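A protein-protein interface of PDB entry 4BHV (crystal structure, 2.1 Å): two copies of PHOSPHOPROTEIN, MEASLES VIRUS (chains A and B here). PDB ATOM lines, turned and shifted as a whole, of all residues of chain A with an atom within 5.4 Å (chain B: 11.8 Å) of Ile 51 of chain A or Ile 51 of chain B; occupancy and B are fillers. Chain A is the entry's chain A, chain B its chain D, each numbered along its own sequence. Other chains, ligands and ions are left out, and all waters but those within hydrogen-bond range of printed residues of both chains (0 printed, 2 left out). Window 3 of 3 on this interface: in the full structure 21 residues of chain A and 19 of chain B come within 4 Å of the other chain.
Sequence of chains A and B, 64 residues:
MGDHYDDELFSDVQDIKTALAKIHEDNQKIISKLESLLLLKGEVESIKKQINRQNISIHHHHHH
Printed residues of chain B within 4 Å of Lys 48 of chain A: Gln 50 (3.2 Å). Printed residues of chain B within 4 Å of Ile 51 of chain A: Ile 47, Gln 50, Ile 51 and Gln 54. No residue of chain B comes within 4 Å of Asn 52 of chain A. Gln 54 of chain A touches one residue of chain B. Of the printed residues of chain A, Ile 47 of chain B touches Ile 51 (3.98 Å). Printed residues of chain A within 4 Å of Gln 50 of chain B: Lys 48 (3.2 Å) and Ile 51 (3.6 Å). Of the printed residues of chain A, Ile 51 of chain B touches Ile 51 (3.97 Å). Of the printed residues of chain A, Gln 54 of chain B touches Ile 51, Gln 54 and Asn 55. His 59 of chain B touches none of the printed residues of chain A. The nearest printed residue of chain A that does not touch Ile 51 of chain B is Ile 47 of chain A (6.6 Å).
OD1 of Asn 55 of chain A sits at hydrogen-bond distance from NE2 of Gln 54 of chain B (3.0 Å). The side-chain amide nitrogen of Gln 50 of chain B lies within hydrogen-bond range of the backbone carbonyl oxygen of Lys 48 of chain A (3.2 Å). The side-chain amide oxygen (OE1) of Gln 54 of chain A sits at hydrogen-bond distance from the side-chain amide nitrogen (NE2) of Gln 54 of chain B, 2.9 Å away.
The backbone carbonyl oxygen (O) of Ile 51 of chain B lies within hydrogen-bond range of the side-chain amide nitrogen (ND2) of Asn 55 of chain B, 3.4 Å away.
Printed residues of chain B that touch a printed residue of chain A: Ile 47, Gln 50, Ile 51 and Gln 54. Hydrophobic or aromatic side chains of chain A that line the printed part of chain B: Ile 51. Along chain A the printed residues that touch a printed residue of chain B span positions 48 to 55. Among the printed residues, 7 pairs touch across the chains. Among the printed residues, no Asp or Glu carboxylate lies within 4 Å of a Lys or Arg side-chain nitrogen of the other chain.
CD1 of Ile 51 of chain A touches CG2 of Ile 47 of chain B (3.98 Å). Gln 50 of chain B touches Ile 51 of chain A (CG to CG2, 3.6 Å). Ile 51 of chain A touches Ile 51 of chain B (CD1 to CG1, 3.97 Å). Ile 51 of chain A touches Gln 54 of chain B (CG2 to NE2, 3.6 Å).
Ile 51 of chain A touches Ile 47 of chain B, but with the chains exchanged Ile 47 of chain A does not touch Ile 51 of chain B (6.6 Å). Ile 51 of chain A touches its own counterpart, Ile 51 of chain B. Ile 51 of chain A touches Gln 54 of chain B, but with the chains exchanged Gln 54 of chain A does not touch Ile 51 of chain B (7.1 Å). Gln 54 of chain A touches its own counterpart, Gln 54 of chain B. 10 positions are printed for both chains.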
ATOM      1  N   SER A  46      13.483  27.211  28.003  1.00  0.00           N
ATOM      2  CA  SER A  46      12.466  27.277  26.973  1.00  0.00           C
ATOM      3  C   SER A  46      13.084  27.210  25.565  1.00  0.00           C
ATOM      4  O   SER A  46      12.514  26.606  24.662  1.00  0.00           O
ATOM      5  CB  SER A  46      11.634  28.535  27.143  1.00  0.00           C
ATOM      6  OG  SER A  46      11.051  28.909  25.923  1.00  0.00           O
ATOM      7  N   ILE A  47      14.240  27.837  25.387  1.00  0.00           N
ATOM      8  CA  ILE A  47      14.961  27.749  24.123  1.00  0.00           C
ATOM      9  C   ILE A  47      15.399  26.309  23.842  1.00  0.00           C
ATOM     10  O   ILE A  47      15.296  25.833  22.723  1.00  0.00           O
ATOM     11  CB  ILE A  47      16.166  28.710  24.078  1.00  0.00           C
ATOM     12  CG1 ILE A  47      15.683  30.156  24.048  1.00  0.00           C
ATOM     13  CG2 ILE A  47      17.038  28.435  22.867  1.00  0.00           C
ATOM     14  CD1 ILE A  47      16.797  31.172  24.047  1.00  0.00           C
ATOM     15  N   LYS A  48      15.860  25.613  24.874  1.00  0.00           N
ATOM     16  CA  LYS A  48      16.318  24.241  24.716  1.00  0.00           C
ATOM     17  C   LYS A  48      15.162  23.362  24.227  1.00  0.00           C
ATOM     18  O   LYS A  48      15.340  22.540  23.335  1.00  0.00           O
ATOM     19  CB  LYS A  48      16.893  23.718  26.047  1.00  0.00           C
ATOM     20  CG  LYS A  48      17.539  22.329  26.006  1.00  0.00           C
ATOM     21  CD  LYS A  48      17.534  21.670  27.389  1.00  0.00           C
ATOM     22  CE  LYS A  48      18.547  20.544  27.513  1.00  0.00           C
ATOM     23  NZ  LYS A  48      19.009  20.320  28.917  1.00  0.00           N
ATOM     24  N   LYS A  49      13.979  23.552  24.804  1.00  0.00           N
ATOM     25  CA  LYS A  49      12.785  22.848  24.354  1.00  0.00           C
ATOM     26  C   LYS A  49      12.383  23.212  22.912  1.00  0.00           C
ATOM     27  O   LYS A  49      12.020  22.342  22.121  1.00  0.00           O
ATOM     28  CB  LYS A  49      11.624  23.087  25.323  1.00  0.00           C
ATOM     29  CG  LYS A  49      11.880  22.553  26.725  1.00  0.00           C
ATOM     30  CD  LYS A  49      10.598  22.366  27.517  1.00  0.00           C
ATOM     31  CE  LYS A  49      10.831  22.521  29.011  1.00  0.00           C
ATOM     32  NZ  LYS A  49      12.114  21.919  29.451  1.00  0.00           N
ATOM     33  N   GLN A  50      12.464  24.498  22.581  1.00  0.00           N
ATOM     34  CA  GLN A  50      12.090  24.983  21.258  1.00  0.00           C
ATOM     35  C   GLN A  50      12.977  24.381  20.176  1.00  0.00           C
ATOM     36  O   GLN A  50      12.500  24.000  19.121  1.00  0.00           O
ATOM     37  CB  GLN A  50      12.149  26.514  21.221  1.00  0.00           C
ATOM     38  CG  GLN A  50      11.595  27.157  19.965  1.00  0.00           C
ATOM     39  CD  GLN A  50      11.686  28.671  19.991  1.00  0.00           C
ATOM     40  OE1 GLN A  50      12.299  29.255  20.877  1.00  0.00           O
ATOM     41  NE2 GLN A  50      11.069  29.311  19.015  1.00  0.00           N
ATOM     42  N   ILE A  51      14.272  24.297  20.453  1.00  0.00           N
ATOM     43  CA  ILE A  51      15.197  23.617  19.560  1.00  0.00           C
ATOM     44  C   ILE A  51      14.867  22.128  19.443  1.00  0.00           C
ATOM     45  O   ILE A  51      14.934  21.569  18.362  1.00  0.00           O
ATOM     46  CB  ILE A  51      16.667  23.828  19.968  1.00  0.00           C
ATOM     47  CG1 ILE A  51      17.003  25.323  19.973  1.00  0.00           C
ATOM     48  CG2 ILE A  51      17.596  23.088  19.017  1.00  0.00           C
ATOM     49  CD1 ILE A  51      18.377  25.640  20.490  1.00  0.00           C
ATOM     50  N   ASN A  52      14.507  21.490  20.551  1.00  0.00           N
ATOM     51  CA  ASN A  52      14.106  20.084  20.502  1.00  0.00           C
ATOM     52  C   ASN A  52      12.840  19.838  19.675  1.00  0.00           C
ATOM     53  O   ASN A  52      12.743  18.841  18.980  1.00  0.00           O
ATOM     54  CB  ASN A  52      13.984  19.441  21.883  1.00  0.00           C
ATOM     55  CG  ASN A  52      13.596  17.973  21.798  1.00  0.00           C
ATOM     56  OD1 ASN A  52      14.395  17.127  21.407  1.00  0.00           O
ATOM     57  ND2 ASN A  52      12.357  17.672  22.143  1.00  0.00           N
ATOM     58  N   ARG A  53      11.887  20.760  19.750  1.00  0.00           N
ATOM     59  CA  ARG A  53      10.657  20.656  18.975  1.00  0.00           C
ATOM     60  C   ARG A  53      10.977  20.681  17.479  1.00  0.00           C
ATOM     61  O   ARG A  53      10.344  19.993  16.692  1.00  0.00           O
ATOM     62  CB  ARG A  53       9.662  21.752  19.353  1.00  0.00           C
ATOM     63  CG  ARG A  53       9.225  21.720  20.812  1.00  0.00           C
ATOM     64  CD  ARG A  53       7.769  22.125  20.984  1.00  0.00           C
ATOM     65  NE  ARG A  53       7.588  23.569  21.115  1.00  0.00           N
ATOM     66  CZ  ARG A  53       8.073  24.310  22.107  1.00  0.00           C
ATOM     67  NH1 ARG A  53       8.792  23.756  23.074  1.00  0.00           N
ATOM     68  NH2 ARG A  53       7.842  25.609  22.124  1.00  0.00           N
ATOM     69  N   GLN A  54      11.979  21.469  17.104  1.00  0.00           N
ATOM     70  CA  GLN A  54      12.428  21.534  15.721  1.00  0.00           C
ATOM     71  C   GLN A  54      12.939  20.170  15.290  1.00  0.00           C
ATOM     72  O   GLN A  54      12.642  19.709  14.201  1.00  0.00           O
ATOM     73  CB  GLN A  54      13.570  22.537  15.588  1.00  0.00           C
ATOM     74  CG  GLN A  54      13.207  23.901  15.042  1.00  0.00           C
ATOM     75  CD  GLN A  54      14.438  24.699  14.647  1.00  0.00           C
ATOM     76  OE1 GLN A  54      15.548  24.382  15.062  1.00  0.00           O
ATOM     77  NE2 GLN A  54      14.244  25.733  13.846  1.00  0.00           N
ATOM     78  N   ASN A  55      13.704  19.528  16.166  1.00  0.00           N
ATOM     79  CA  ASN A  55      14.250  18.214  15.877  1.00  0.00           C
ATOM     80  C   ASN A  55      13.140  17.182  15.672  1.00  0.00           C
ATOM     81  O   ASN A  55      13.197  16.368  14.762  1.00  0.00           O
ATOM     82  CB  ASN A  55      15.193  17.772  16.992  1.00  0.00           C
ATOM     83  CG  ASN A  55      16.478  18.586  17.039  1.00  0.00           C
ATOM     84  OD1 ASN A  55      16.899  19.167  16.047  1.00  0.00           O
ATOM     85  ND2 ASN A  55      17.101  18.626  18.201  1.00  0.00           N
ATOM     86  N   GLY B  42      26.998  27.738  31.633  1.00  0.00           N
ATOM     87  CA  GLY B  42      26.832  26.375  31.166  1.00  0.00           C
ATOM     88  C   GLY B  42      25.616  26.146  30.284  1.00  0.00           C
ATOM     89  O   GLY B  42      25.690  25.407  29.320  1.00  0.00           O
ATOM     90  N   GLU B  43      24.490  26.760  30.633  1.00  0.00           N
ATOM     91  CA  GLU B  43      23.263  26.625  29.848  1.00  0.00           C
ATOM     92  C   GLU B  43      23.375  27.197  28.438  1.00  0.00           C
ATOM     93  O   GLU B  43      22.934  26.574  27.484  1.00  0.00           O
ATOM     94  CB  GLU B  43      22.092  27.286  30.571  1.00  0.00           C
ATOM     95  CG  GLU B  43      21.693  26.595  31.861  1.00  0.00           C
ATOM     96  CD  GLU B  43      21.582  25.100  31.692  1.00  0.00           C
ATOM     97  OE1 GLU B  43      20.680  24.642  30.971  1.00  0.00           O
ATOM     98  OE2 GLU B  43      22.410  24.379  32.268  1.00  0.00           O
ATOM     99  N   VAL B  44      23.966  28.379  28.313  1.00  0.00           N
ATOM    100  CA  VAL B  44      24.165  28.985  27.009  1.00  0.00           C
ATOM    101  C   VAL B  44      25.082  28.091  26.166  1.00  0.00           C
ATOM    102  O   VAL B  44      24.860  27.911  24.979  1.00  0.00           O
ATOM    103  CB  VAL B  44      24.717  30.426  27.112  1.00  0.00           C
ATOM    104  CG1 VAL B  44      25.118  30.943  25.746  1.00  0.00           C
ATOM    105  CG2 VAL B  44      23.696  31.355  27.739  1.00  0.00           C
ATOM    106  N   GLU B  45      26.091  27.511  26.809  1.00  0.00           N
ATOM    107  CA  GLU B  45      27.012  26.578  26.163  1.00  0.00           C
ATOM    108  C   GLU B  45      26.301  25.314  25.679  1.00  0.00           C
ATOM    109  O   GLU B  45      26.612  24.802  24.610  1.00  0.00           O
ATOM    110  CB  GLU B  45      28.168  26.224  27.091  1.00  0.00           C
ATOM    111  CG  GLU B  45      29.418  25.731  26.383  1.00  0.00           C
ATOM    112  CD  GLU B  45      30.081  26.811  25.553  1.00  0.00           C
ATOM    113  OE1 GLU B  45      30.463  27.850  26.116  1.00  0.00           O
ATOM    114  OE2 GLU B  45      30.201  26.625  24.330  1.00  0.00           O
ATOM    115  N   SER B  46      25.332  24.839  26.456  1.00  0.00           N
ATOM    116  CA  SER B  46      24.539  23.665  26.086  1.00  0.00           C
ATOM    117  C   SER B  46      23.785  23.930  24.791  1.00  0.00           C
ATOM    118  O   SER B  46      23.714  23.066  23.928  1.00  0.00           O
ATOM    119  CB  SER B  46      23.519  23.323  27.178  1.00  0.00           C
ATOM    120  OG  SER B  46      24.090  22.555  28.217  1.00  0.00           O
ATOM    121  N   ILE B  47      23.231  25.131  24.669  1.00  0.00           N
ATOM    122  CA  ILE B  47      22.520  25.531  23.466  1.00  0.00           C
ATOM    123  C   ILE B  47      23.439  25.572  22.241  1.00  0.00           C
ATOM    124  O   ILE B  47      23.044  25.158  21.163  1.00  0.00           O
ATOM    125  CB  ILE B  47      21.771  26.869  23.648  1.00  0.00           C
ATOM    126  CG1 ILE B  47      20.514  26.655  24.485  1.00  0.00           C
ATOM    127  CG2 ILE B  47      21.401  27.482  22.309  1.00  0.00           C
ATOM    128  CD1 ILE B  47      20.153  27.832  25.350  1.00  0.00           C
ATOM    129  N   LYS B  48      24.668  26.045  22.417  1.00  0.00           N
ATOM    130  CA  LYS B  48      25.595  26.108  21.290  1.00  0.00           C
ATOM    131  C   LYS B  48      25.860  24.703  20.743  1.00  0.00           C
ATOM    132  O   LYS B  48      25.837  24.499  19.536  1.00  0.00           O
ATOM    133  CB  LYS B  48      26.909  26.797  21.691  1.00  0.00           C
ATOM    134  CG  LYS B  48      27.876  27.053  20.541  1.00  0.00           C
ATOM    135  CD  LYS B  48      29.082  27.859  20.993  1.00  0.00           C
ATOM    136  CE  LYS B  48      30.278  27.650  20.074  1.00  0.00           C
ATOM    137  NZ  LYS B  48      31.374  28.624  20.339  1.00  0.00           N
ATOM    138  N   LYS B  49      26.082  23.744  21.639  1.00  0.00           N
ATOM    139  CA  LYS B  49      26.240  22.336  21.269  1.00  0.00           C
ATOM    140  C   LYS B  49      24.979  21.726  20.628  1.00  0.00           C
ATOM    141  O   LYS B  49      25.069  20.973  19.660  1.00  0.00           O
ATOM    142  CB  LYS B  49      26.676  21.493  22.473  1.00  0.00           C
ATOM    143  CG  LYS B  49      28.109  21.728  22.933  1.00  0.00           C
ATOM    144  CD  LYS B  49      28.555  20.667  23.930  1.00  0.00           C
ATOM    145  CE  LYS B  49      29.926  20.977  24.501  1.00  0.00           C
ATOM    146  NZ  LYS B  49      29.869  22.050  25.528  1.00  0.00           N
ATOM    147  N   GLN B  50      23.813  22.068  21.164  1.00  0.00           N
ATOM    148  CA  GLN B  50      22.550  21.563  20.649  1.00  0.00           C
ATOM    149  C   GLN B  50      22.351  22.012  19.202  1.00  0.00           C
ATOM    150  O   GLN B  50      21.923  21.236  18.363  1.00  0.00           O
ATOM    151  CB  GLN B  50      21.403  22.057  21.538  1.00  0.00           C
ATOM    152  CG  GLN B  50      20.007  21.579  21.181  1.00  0.00           C
ATOM    153  CD  GLN B  50      18.983  21.929  22.254  1.00  0.00           C
ATOM    154  OE1 GLN B  50      19.041  22.989  22.862  1.00  0.00           O
ATOM    155  NE2 GLN B  50      18.042  21.027  22.487  1.00  0.00           N
ATOM    156  N   ILE B  51      22.676  23.266  18.908  1.00  0.00           N
ATOM    157  CA  ILE B  51      22.614  23.759  17.536  1.00  0.00           C
ATOM    158  C   ILE B  51      23.609  23.031  16.609  1.00  0.00           C
ATOM    159  O   ILE B  51      23.279  22.686  15.482  1.00  0.00           O
ATOM    160  CB  ILE B  51      22.773  25.291  17.475  1.00  0.00           C
ATOM    161  CG1 ILE B  51      21.652  25.955  18.276  1.00  0.00           C
ATOM    162  CG2 ILE B  51      22.750  25.782  16.039  1.00  0.00           C
ATOM    163  CD1 ILE B  51      21.710  27.460  18.318  1.00  0.00           C
ATOM    164  N   ASN B  52      24.815  22.774  17.100  1.00  0.00           N
ATOM    165  CA  ASN B  52      25.798  22.039  16.311  1.00  0.00           C
ATOM    166  C   ASN B  52      25.325  20.625  15.989  1.00  0.00           C
ATOM    167  O   ASN B  52      25.544  20.136  14.891  1.00  0.00           O
ATOM    168  CB  ASN B  52      27.177  22.024  16.973  1.00  0.00           C
ATOM    169  CG  ASN B  52      28.243  21.402  16.085  1.00  0.00           C
ATOM    170  OD1 ASN B  52      28.393  21.768  14.924  1.00  0.00           O
ATOM    171  ND2 ASN B  52      28.978  20.446  16.633  1.00  0.00           N
ATOM    172  N   ARG B  53      24.643  19.991  16.940  1.00  0.00           N
ATOM    173  CA  ARG B  53      24.124  18.638  16.748  1.00  0.00           C
ATOM    174  C   ARG B  53      23.119  18.608  15.603  1.00  0.00           C
ATOM    175  O   ARG B  53      23.083  17.659  14.828  1.00  0.00           O
ATOM    176  CB  ARG B  53      23.475  18.103  18.026  1.00  0.00           C
ATOM    177  CG  ARG B  53      24.447  17.521  19.039  1.00  0.00           C
ATOM    178  CD  ARG B  53      23.770  16.497  19.938  1.00  0.00           C
ATOM    179  NE  ARG B  53      22.766  17.073  20.830  1.00  0.00           N
ATOM    180  CZ  ARG B  53      23.034  17.725  21.960  1.00  0.00           C
ATOM    181  NH1 ARG B  53      24.279  17.910  22.359  1.00  0.00           N
ATOM    182  NH2 ARG B  53      22.048  18.198  22.695  1.00  0.00           N
ATOM    183  N   GLN B  54      22.318  19.663  15.501  1.00  0.00           N
ATOM    184  CA  GLN B  54      21.350  19.793  14.423  1.00  0.00           C
ATOM    185  C   GLN B  54      22.081  19.820  13.094  1.00  0.00           C
ATOM    186  O   GLN B  54      21.683  19.163  12.140  1.00  0.00           O
ATOM    187  CB  GLN B  54      20.600  21.114  14.555  1.00  0.00           C
ATOM    188  CG  GLN B  54      19.432  21.120  15.510  1.00  0.00           C
ATOM    189  CD  GLN B  54      18.496  22.277  15.235  1.00  0.00           C
ATOM    190  OE1 GLN B  54      18.914  23.321  14.734  1.00  0.00           O
ATOM    191  NE2 GLN B  54      17.226  22.101  15.560  1.00  0.00           N
ATOM    192  N   ASN B  55      23.160  20.591  13.044  1.00  0.00           N
ATOM    193  CA  ASN B  55      23.931  20.747  11.823  1.00  0.00           C
ATOM    194  C   ASN B  55      24.517  19.417  11.363  1.00  0.00           C
ATOM    195  O   ASN B  55      24.528  19.113  10.174  1.00  0.00           O
ATOM    196  CB  ASN B  55      25.037  21.783  12.025  1.00  0.00           C
ATOM    197  CG  ASN B  55      24.490  23.180  12.269  1.00  0.00           C
ATOM    198  OD1 ASN B  55      23.425  23.540  11.784  1.00  0.00           O
ATOM    199  ND2 ASN B  55      25.228  23.970  13.023  1.00  0.00           N
ATOM    200  N   ILE B  56      25.003  18.631  12.317  1.00  0.00           N
ATOM    201  CA  ILE B  56      25.482  17.288  12.027  1.00  0.00           C
ATOM    202  C   ILE B  56      24.383  16.334  11.531  1.00  0.00           C
ATOM    203  O   ILE B  56      24.595  15.588  10.581  1.00  0.00           O
ATOM    204  CB  ILE B  56      26.166  16.662  13.247  1.00  0.00           C
ATOM    205  CG1 ILE B  56      27.497  17.356  13.522  1.00  0.00           C
ATOM    206  CG2 ILE B  56      26.361  15.171  13.027  1.00  0.00           C
ATOM    207  CD1 ILE B  56      27.947  17.266  14.957  1.00  0.00           C
ATOM    208  N   SER B  57      23.219  16.363  12.180  1.00  0.00           N
ATOM    209  CA  SER B  57      22.112  15.491  11.789  1.00  0.00           C
ATOM    210  C   SER B  57      21.720  15.844  10.368  1.00  0.00           C
ATOM    211  O   SER B  57      21.495  14.974   9.534  1.00  0.00           O
ATOM    212  CB  SER B  57      20.886  15.691  12.696  1.00  0.00           C
ATOM    213  OG  SER B  57      21.126  15.335  14.039  1.00  0.00           O
ATOM    214  N   ILE B  58      21.662  17.142  10.107  1.00  0.00           N
ATOM    215  CA  ILE B  58      21.277  17.660   8.810  1.00  0.00           C
ATOM    216  C   ILE B  58      22.250  17.199   7.729  1.00  0.00           C
ATOM    217  O   ILE B  58      21.835  16.855   6.633  1.00  0.00           O
ATOM    218  CB  ILE B  58      21.247  19.197   8.828  1.00  0.00           C
ATOM    219  CG1 ILE B  58      19.902  19.702   9.342  1.00  0.00           C
ATOM    220  CG2 ILE B  58      21.551  19.750   7.446  1.00  0.00           C
ATOM    221  CD1 ILE B  58      19.730  21.200   9.240  1.00  0.00           C
ATOM    222  N   HIS B  59      23.543  17.205   8.039  1.00  0.00           N
ATOM    223  CA  HIS B  59      24.548  16.766   7.083  1.00  0.00           C
ATOM    224  C   HIS B  59      24.395  15.291   6.725  1.00  0.00           C
ATOM    225  O   HIS B  59      24.476  14.925   5.562  1.00  0.00           O
ATOM    226  CB  HIS B  59      25.955  17.031   7.621  1.00  0.00           C
ATOM    227  CG  HIS B  59      27.020  16.224   6.948  1.00  0.00           C
ATOM    228  ND1 HIS B  59      27.565  15.092   7.511  1.00  0.00           N
ATOM    229  CD2 HIS B  59      27.633  16.382   5.753  1.00  0.00           C
ATOM    230  CE1 HIS B  59      28.470  14.588   6.692  1.00  0.00           C
ATOM    231  NE2 HIS B  59      28.529  15.352   5.617  1.00  0.00           N
ATOM    232  N   HIS B  60      24.180  14.450   7.730  1.00  0.00           N
ATOM    233  CA  HIS B  60      23.932  13.027   7.509  1.00  0.00           C
ATOM    234  C   HIS B  60      22.557  12.870   6.860  1.00  0.00           C
ATOM    235  O   HIS B  60      22.342  12.013   6.008  1.00  0.00           O
ATOM    236  CB  HIS B  60      23.944  12.258   8.831  1.00  0.00           C
ATOM    237  CG  HIS B  60      25.311  11.972   9.369  1.00  0.00           C
ATOM    238  ND1 HIS B  60      25.894  12.732  10.357  1.00  0.00           N
ATOM    239  CD2 HIS B  60      26.194  10.989   9.081  1.00  0.00           C
ATOM    240  CE1 HIS B  60      27.083  12.239  10.646  1.00  0.00           C
ATOM    241  NE2 HIS B  60      27.290  11.180   9.887  1.00  0.00           N
